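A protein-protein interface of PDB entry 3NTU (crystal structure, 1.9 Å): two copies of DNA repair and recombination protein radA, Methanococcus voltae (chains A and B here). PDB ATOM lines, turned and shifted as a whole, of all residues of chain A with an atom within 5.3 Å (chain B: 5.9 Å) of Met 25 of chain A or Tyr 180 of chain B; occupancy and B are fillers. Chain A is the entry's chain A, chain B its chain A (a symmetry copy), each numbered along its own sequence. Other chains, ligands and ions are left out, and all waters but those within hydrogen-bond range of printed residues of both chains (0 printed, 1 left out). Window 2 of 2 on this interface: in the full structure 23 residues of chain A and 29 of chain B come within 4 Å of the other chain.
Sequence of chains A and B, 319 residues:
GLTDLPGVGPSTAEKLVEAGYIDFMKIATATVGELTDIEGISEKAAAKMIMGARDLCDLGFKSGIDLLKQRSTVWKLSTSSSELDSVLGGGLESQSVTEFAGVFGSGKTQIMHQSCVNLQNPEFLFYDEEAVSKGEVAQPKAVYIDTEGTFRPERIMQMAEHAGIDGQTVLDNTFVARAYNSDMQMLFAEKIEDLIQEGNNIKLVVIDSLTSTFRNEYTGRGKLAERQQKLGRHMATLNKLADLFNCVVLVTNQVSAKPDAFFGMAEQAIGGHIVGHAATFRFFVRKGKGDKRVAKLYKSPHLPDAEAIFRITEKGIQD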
ATOM      1  N   ASP A  23     -21.135  -4.820  -1.525  1.00  0.00           N
ATOM      2  CA  ASP A  23     -20.224  -4.388  -2.574  1.00  0.00           C
ATOM      3  C   ASP A  23     -18.823  -4.172  -2.026  1.00  0.00           C
ATOM      4  O   ASP A  23     -18.616  -4.049  -0.815  1.00  0.00           O
ATOM      5  CB  ASP A  23     -20.715  -3.153  -3.331  1.00  0.00           C
ATOM      6  CG  ASP A  23     -20.892  -1.943  -2.451  1.00  0.00           C
ATOM      7  OD1 ASP A  23     -20.275  -1.892  -1.365  1.00  0.00           O
ATOM      8  OD2 ASP A  23     -21.643  -1.027  -2.868  1.00  0.00           O
ATOM      9  N   PHE A  24     -17.863  -4.142  -2.930  1.00  0.00           N
ATOM     10  CA  PHE A  24     -16.477  -4.028  -2.536  1.00  0.00           C
ATOM     11  C   PHE A  24     -16.085  -2.803  -1.724  1.00  0.00           C
ATOM     12  O   PHE A  24     -15.287  -2.929  -0.792  1.00  0.00           O
ATOM     13  CB  PHE A  24     -15.613  -4.133  -3.771  1.00  0.00           C
ATOM     14  CG  PHE A  24     -15.720  -5.461  -4.471  1.00  0.00           C
ATOM     15  CD1 PHE A  24     -15.321  -5.598  -5.792  1.00  0.00           C
ATOM     16  CD2 PHE A  24     -16.215  -6.579  -3.808  1.00  0.00           C
ATOM     17  CE1 PHE A  24     -15.421  -6.851  -6.436  1.00  0.00           C
ATOM     18  CE2 PHE A  24     -16.310  -7.819  -4.449  1.00  0.00           C
ATOM     19  CZ  PHE A  24     -15.918  -7.947  -5.745  1.00  0.00           C
ATOM     20  N   MET A  25     -16.613  -1.624  -2.067  1.00  0.00           N
ATOM     21  CA  MET A  25     -16.220  -0.437  -1.314  1.00  0.00           C
ATOM     22  C   MET A  25     -16.558  -0.529   0.147  1.00  0.00           C
ATOM     23  O   MET A  25     -15.786  -0.076   0.997  1.00  0.00           O
ATOM     24  CB  MET A  25     -16.813   0.837  -1.928  1.00  0.00           C
ATOM     25  CG  MET A  25     -15.973   1.398  -3.066  1.00  0.00           C
ATOM     26  SD  MET A  25     -14.244   1.751  -2.544  1.00  0.00           S
ATOM     27  CE  MET A  25     -14.550   3.079  -1.383  1.00  0.00           C
ATOM     28  N   LYS A  26     -17.688  -1.131   0.477  1.00  0.00           N
ATOM     29  CA  LYS A  26     -18.046  -1.230   1.873  1.00  0.00           C
ATOM     30  C   LYS A  26     -17.079  -2.163   2.570  1.00  0.00           C
ATOM     31  O   LYS A  26     -16.754  -1.977   3.748  1.00  0.00           O
ATOM     32  CB  LYS A  26     -19.471  -1.721   2.069  1.00  0.00           C
ATOM     33  CG  LYS A  26     -19.884  -1.648   3.524  1.00  0.00           C
ATOM     34  CD  LYS A  26     -21.357  -1.959   3.774  1.00  0.00           C
ATOM     35  CE  LYS A  26     -21.713  -1.654   5.242  1.00  0.00           C
ATOM     36  NZ  LYS A  26     -23.031  -2.226   5.653  1.00  0.00           N
ATOM     37  N   ILE A  27     -16.621  -3.190   1.863  1.00  0.00           N
ATOM     38  CA  ILE A  27     -15.657  -4.080   2.492  1.00  0.00           C
ATOM     39  C   ILE A  27     -14.273  -3.449   2.590  1.00  0.00           C
ATOM     40  O   ILE A  27     -13.576  -3.644   3.582  1.00  0.00           O
ATOM     41  CB  ILE A  27     -15.523  -5.413   1.724  1.00  0.00           C
ATOM     42  CG1 ILE A  27     -16.804  -6.225   1.937  1.00  0.00           C
ATOM     43  CG2 ILE A  27     -14.334  -6.211   2.276  1.00  0.00           C
ATOM     44  CD1 ILE A  27     -16.936  -7.432   1.008  1.00  0.00           C
ATOM     45  N   ALA A  28     -13.886  -2.717   1.552  1.00  0.00           N
ATOM     46  CA  ALA A  28     -12.585  -2.062   1.491  1.00  0.00           C
ATOM     47  C   ALA A  28     -12.422  -1.003   2.624  1.00  0.00           C
ATOM     48  O   ALA A  28     -11.309  -0.773   3.115  1.00  0.00           O
ATOM     49  CB  ALA A  28     -12.418  -1.412   0.118  1.00  0.00           C
ATOM     50  N   THR A  29     -13.555  -0.442   3.075  1.00  0.00           N
ATOM     51  CA  THR A  29     -13.580   0.582   4.111  1.00  0.00           C
ATOM     52  C   THR A  29     -14.061   0.089   5.459  1.00  0.00           C
ATOM     53  O   THR A  29     -14.389   0.892   6.333  1.00  0.00           O
ATOM     54  CB  THR A  29     -14.453   1.787   3.669  1.00  0.00           C
ATOM     55  OG1 THR A  29     -15.828   1.399   3.573  1.00  0.00           O
ATOM     56  CG2 THR A  29     -14.012   2.287   2.332  1.00  0.00           C
ATOM     57  N   ALA A  30     -14.089  -1.229   5.647  1.00  0.00           N
ATOM     58  CA  ALA A  30     -14.515  -1.818   6.910  1.00  0.00           C
ATOM     59  C   ALA A  30     -13.309  -2.008   7.841  1.00  0.00           C
ATOM     60  O   ALA A  30     -12.160  -1.915   7.393  1.00  0.00           O
ATOM     61  CB  ALA A  30     -15.181  -3.190   6.644  1.00  0.00           C
ATOM     62  N   CYS A  57     -10.472  -2.287  -5.787  1.00  0.00           N
ATOM     63  CA  CYS A  57     -11.044  -0.956  -6.007  1.00  0.00           C
ATOM     64  C   CYS A  57      -9.964   0.084  -6.340  1.00  0.00           C
ATOM     65  O   CYS A  57     -10.271   1.252  -6.538  1.00  0.00           O
ATOM     66  CB  CYS A  57     -11.843  -0.515  -4.771  1.00  0.00           C
ATOM     67  SG  CYS A  57     -13.380  -1.456  -4.475  1.00  0.00           S
ATOM     68  N   LEU A  59      -7.555   1.486  -4.449  1.00  0.00           N
ATOM     69  CA  LEU A  59      -7.474   2.558  -3.463  1.00  0.00           C
ATOM     70  C   LEU A  59      -6.043   2.839  -3.001  1.00  0.00           C
ATOM     71  O   LEU A  59      -5.709   2.592  -1.834  1.00  0.00           O
ATOM     72  CB  LEU A  59      -8.321   2.200  -2.245  1.00  0.00           C
ATOM     73  CG  LEU A  59      -9.784   1.874  -2.513  1.00  0.00           C
ATOM     74  CD1 LEU A  59     -10.453   1.635  -1.177  1.00  0.00           C
ATOM     75  CD2 LEU A  59     -10.470   3.005  -3.265  1.00  0.00           C
ATOM     76  N   ASP A 243     -20.346   9.584   0.081  1.00  0.00           N
ATOM     77  CA  ASP A 243     -19.150   9.131  -0.632  1.00  0.00           C
ATOM     78  C   ASP A 243     -19.348   7.764  -1.301  1.00  0.00           C
ATOM     79  O   ASP A 243     -19.124   7.610  -2.505  1.00  0.00           O
ATOM     80  CB  ASP A 243     -17.971   8.998   0.342  1.00  0.00           C
ATOM     81  CG  ASP A 243     -17.427  10.333   0.829  1.00  0.00           C
ATOM     82  OD1 ASP A 243     -17.858  11.406   0.339  1.00  0.00           O
ATOM     83  OD2 ASP A 243     -16.533  10.300   1.715  1.00  0.00           O
ATOM     84  N   LEU A 244     -19.765   6.778  -0.527  1.00  0.00           N
ATOM     85  CA  LEU A 244     -19.899   5.426  -1.068  1.00  0.00           C
ATOM     86  C   LEU A 244     -20.979   5.247  -2.104  1.00  0.00           C
ATOM     87  O   LEU A 244     -20.830   4.442  -3.022  1.00  0.00           O
ATOM     88  CB  LEU A 244     -20.102   4.398   0.052  1.00  0.00           C
ATOM     89  CG  LEU A 244     -18.808   3.664   0.466  1.00  0.00           C
ATOM     90  CD1 LEU A 244     -17.674   4.671   0.691  1.00  0.00           C
ATOM     91  CD2 LEU A 244     -19.077   2.826   1.729  1.00  0.00           C
ATOM     92  N   ASP B 146      -5.583  12.373   2.297  1.00  0.00           N
ATOM     93  CA  ASP B 146      -6.857  13.042   2.445  1.00  0.00           C
ATOM     94  C   ASP B 146      -7.843  12.126   3.146  1.00  0.00           C
ATOM     95  O   ASP B 146      -8.346  11.165   2.548  1.00  0.00           O
ATOM     96  CB  ASP B 146      -7.352  13.369   1.028  1.00  0.00           C
ATOM     97  CG  ASP B 146      -8.707  14.024   1.006  1.00  0.00           C
ATOM     98  OD1 ASP B 146      -9.211  14.410   2.081  1.00  0.00           O
ATOM     99  OD2 ASP B 146      -9.273  14.162  -0.116  1.00  0.00           O
ATOM    100  N   THR B 147      -8.149  12.427   4.392  1.00  0.00           N
ATOM    101  CA  THR B 147      -9.076  11.555   5.126  1.00  0.00           C
ATOM    102  C   THR B 147     -10.500  12.095   5.119  1.00  0.00           C
ATOM    103  O   THR B 147     -11.367  11.501   5.741  1.00  0.00           O
ATOM    104  CB  THR B 147      -8.670  11.352   6.602  1.00  0.00           C
ATOM    105  OG1 THR B 147      -8.968  12.540   7.349  1.00  0.00           O
ATOM    106  CG2 THR B 147      -7.157  11.026   6.702  1.00  0.00           C
ATOM    107  N   ARG B 178      -6.723   8.741  -0.747  1.00  0.00           N
ATOM    108  CA  ARG B 178      -7.970   8.981  -0.006  1.00  0.00           C
ATOM    109  C   ARG B 178      -8.155   7.835   1.005  1.00  0.00           C
ATOM    110  O   ARG B 178      -8.284   6.666   0.613  1.00  0.00           O
ATOM    111  CB  ARG B 178      -9.178   8.992  -0.964  1.00  0.00           C
ATOM    112  CG  ARG B 178     -10.534   9.081  -0.268  1.00  0.00           C
ATOM    113  CD  ARG B 178     -10.920  10.530   0.067  1.00  0.00           C
ATOM    114  NE  ARG B 178     -12.270  10.548   0.620  1.00  0.00           N
ATOM    115  CZ  ARG B 178     -12.503  10.319   1.894  1.00  0.00           C
ATOM    116  NH1 ARG B 178     -11.479  10.102   2.675  1.00  0.00           N
ATOM    117  NH2 ARG B 178     -13.729  10.261   2.379  1.00  0.00           N
ATOM    118  N   ALA B 179      -8.143   8.179   2.294  1.00  0.00           N
ATOM    119  CA  ALA B 179      -8.333   7.235   3.411  1.00  0.00           C
ATOM    120  C   ALA B 179      -9.745   7.418   3.963  1.00  0.00           C
ATOM    121  O   ALA B 179     -10.148   8.538   4.288  1.00  0.00           O
ATOM    122  CB  ALA B 179      -7.309   7.508   4.510  1.00  0.00           C
ATOM    123  N   TYR B 180     -10.500   6.329   4.088  1.00  0.00           N
ATOM    124  CA  TYR B 180     -11.876   6.412   4.574  1.00  0.00           C
ATOM    125  C   TYR B 180     -11.949   6.108   6.066  1.00  0.00           C
ATOM    126  O   TYR B 180     -12.987   6.273   6.695  1.00  0.00           O
ATOM    127  CB  TYR B 180     -12.727   5.432   3.764  1.00  0.00           C
ATOM    128  CG  TYR B 180     -12.886   5.838   2.303  1.00  0.00           C
ATOM    129  CD1 TYR B 180     -13.960   6.641   1.889  1.00  0.00           C
ATOM    130  CD2 TYR B 180     -11.954   5.442   1.350  1.00  0.00           C
ATOM    131  CE1 TYR B 180     -14.083   7.030   0.534  1.00  0.00           C
ATOM    132  CE2 TYR B 180     -12.062   5.816   0.013  1.00  0.00           C
ATOM    133  CZ  TYR B 180     -13.121   6.606  -0.391  1.00  0.00           C
ATOM    134  OH  TYR B 180     -13.195   6.975  -1.699  1.00  0.00           O
ATOM    135  N   ASN B 181     -10.835   5.673   6.649  1.00  0.00           N
ATOM    136  CA  ASN B 181     -10.828   5.374   8.097  1.00  0.00           C
ATOM    137  C   ASN B 181      -9.411   5.398   8.619  1.00  0.00           C
ATOM    138  O   ASN B 181      -8.473   5.499   7.842  1.00  0.00           O
ATOM    139  CB  ASN B 181     -11.456   4.003   8.382  1.00  0.00           C
ATOM    140  CG  ASN B 181     -10.796   2.898   7.595  1.00  0.00           C
ATOM    141  OD1 ASN B 181     -11.479   2.033   7.012  1.00  0.00           O
ATOM    142  ND2 ASN B 181      -9.473   2.891   7.570  1.00  0.00           N
ATOM    143  N   SER B 182      -9.256   5.310   9.940  1.00  0.00           N
ATOM    144  CA  SER B 182      -7.905   5.405  10.549  1.00  0.00           C
ATOM    145  C   SER B 182      -6.955   4.305  10.112  1.00  0.00           C
ATOM    146  O   SER B 182      -5.763   4.541   9.994  1.00  0.00           O
ATOM    147  CB  SER B 182      -8.036   5.451  12.081  1.00  0.00           C
ATOM    148  OG  SER B 182      -8.435   4.208  12.594  1.00  0.00           O
ATOM    149  N   MET B 184      -6.722   2.879   7.086  1.00  0.00           N
ATOM    150  CA  MET B 184      -6.189   3.245   5.775  1.00  0.00           C
ATOM    151  C   MET B 184      -5.204   4.392   5.909  1.00  0.00           C
ATOM    152  O   MET B 184      -4.131   4.412   5.287  1.00  0.00           O
ATOM    153  CB  MET B 184      -7.354   3.690   4.857  1.00  0.00           C
ATOM    154  CG  MET B 184      -8.266   2.525   4.448  1.00  0.00           C
ATOM    155  SD  MET B 184      -9.560   3.024   3.267  1.00  0.00           S
ATOM    156  CE  MET B 184      -8.548   3.316   1.827  1.00  0.00           C
ATOM    157  N   GLN B 185      -5.626   5.386   6.678  1.00  0.00           N
ATOM    158  CA  GLN B 185      -4.794   6.570   6.944  1.00  0.00           C
ATOM    159  C   GLN B 185      -3.391   6.131   7.429  1.00  0.00           C
ATOM    160  O   GLN B 185      -2.345   6.541   6.896  1.00  0.00           O
ATOM    161  CB  GLN B 185      -5.484   7.411   8.036  1.00  0.00           C
ATOM    162  CG  GLN B 185      -4.700   8.645   8.502  1.00  0.00           C
ATOM    163  CD  GLN B 185      -5.465   9.418   9.555  1.00  0.00           C
ATOM    164  OE1 GLN B 185      -6.714   9.302   9.672  1.00  0.00           O
ATOM    165  NE2 GLN B 185      -4.752  10.229  10.316  1.00  0.00           N
ATOM    166  N   THR B 213     -10.831  10.861  11.550  1.00  0.00           N
ATOM    167  CA  THR B 213     -11.171   9.435  11.461  1.00  0.00           C
ATOM    168  C   THR B 213     -11.194   8.811  12.882  1.00  0.00           C
ATOM    169  O   THR B 213     -12.213   8.258  13.314  1.00  0.00           O
ATOM    170  CB  THR B 213     -10.163   8.660  10.600  1.00  0.00           C
ATOM    171  OG1 THR B 213      -8.841   8.861  11.119  1.00  0.00           O
ATOM    172  CG2 THR B 213     -10.217   9.148   9.130  1.00  0.00           C
ATOM    173  N   GLU B 217     -14.367   7.004  15.167  1.00  0.00           N
ATOM    174  CA  GLU B 217     -14.265   5.541  15.230  1.00  0.00           C
ATOM    175  C   GLU B 217     -14.136   5.021  16.653  1.00  0.00           C
ATOM    176  O   GLU B 217     -14.490   3.881  16.935  1.00  0.00           O
ATOM    177  CB  GLU B 217     -13.049   5.028  14.485  1.00  0.00           C
ATOM    178  CG  GLU B 217     -13.055   5.353  13.034  1.00  0.00           C
ATOM    179  CD  GLU B 217     -11.759   4.972  12.363  1.00  0.00           C
ATOM    180  OE1 GLU B 217     -11.566   5.372  11.211  1.00  0.00           O
ATOM    181  OE2 GLU B 217     -10.934   4.273  12.988  1.00  0.00           O
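OD1 of Asn 181 of chain B lies close to O of Thr 29 of chain A, at 3.2 Å.
The side-chain carboxylate (OD2) of Asp 243 of chain A is in salt-bridge range of the guanidinium group (NH2) of Arg 178 of chain B (2.9 Å).
The backbone NH (N) of Met 184 of chain B sits close to the side-chain amide nitrogen (ND2) of Asn 181 of chain B (2.8 Å).
The backbone carbonyl oxygen (O) of Met 25 of chain A lies within hydrogen-bond range of the side-chain hydroxyl (OG1) of Thr 29 of chain A.
The backbone carbonyl oxygen (O) of Asp 146 of chain B lies within hydrogen-bond range of the guanidinium group (NH1) of Arg 178 of chain B (3.3 Å).
The guanidinium group of Arg 178 of chain B lies close to the backbone carbonyl oxygen of Thr 147 of chain B (3.4 Å).
The backbone NH (N) of Tyr 180 of chain B sits at hydrogen-bond distance from the side-chain sulfur (SD) of Met 184 of chain B (3.5 Å).
Tyr 180 of chain B touches Met 25 of chain A.
CG2 of Thr 29 of chain A touches CB of Tyr 180 of chain B (3.7 Å).
Met 184 of chain B touches Leu 59 of chain A.
Of chain B, only Tyr 180 (3.9 Å) comes within 4 Å of Met 25 of chain A.
Of chain A, only Met 25 (3.9 Å) and Thr 29 (3.7 Å) come within 4 Å of Tyr 180 of chain B.
Of the printed residues of chain A, Arg 178 of chain B touches Asp 243 (2.9 Å).
Of the printed residues of chain B, Leu 59 of chain A touches Met 184 (3.9 Å).
Asp 23 of chain A touches none of the printed residues of chain B.
The nearest residue of chain A that does not touch Tyr 180 of chain B is Asp 243 of chain A (4.3 Å).
Along chain A the printed residues that touch a printed residue of chain B span positions 25 to 243.
No position is printed for both chains.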
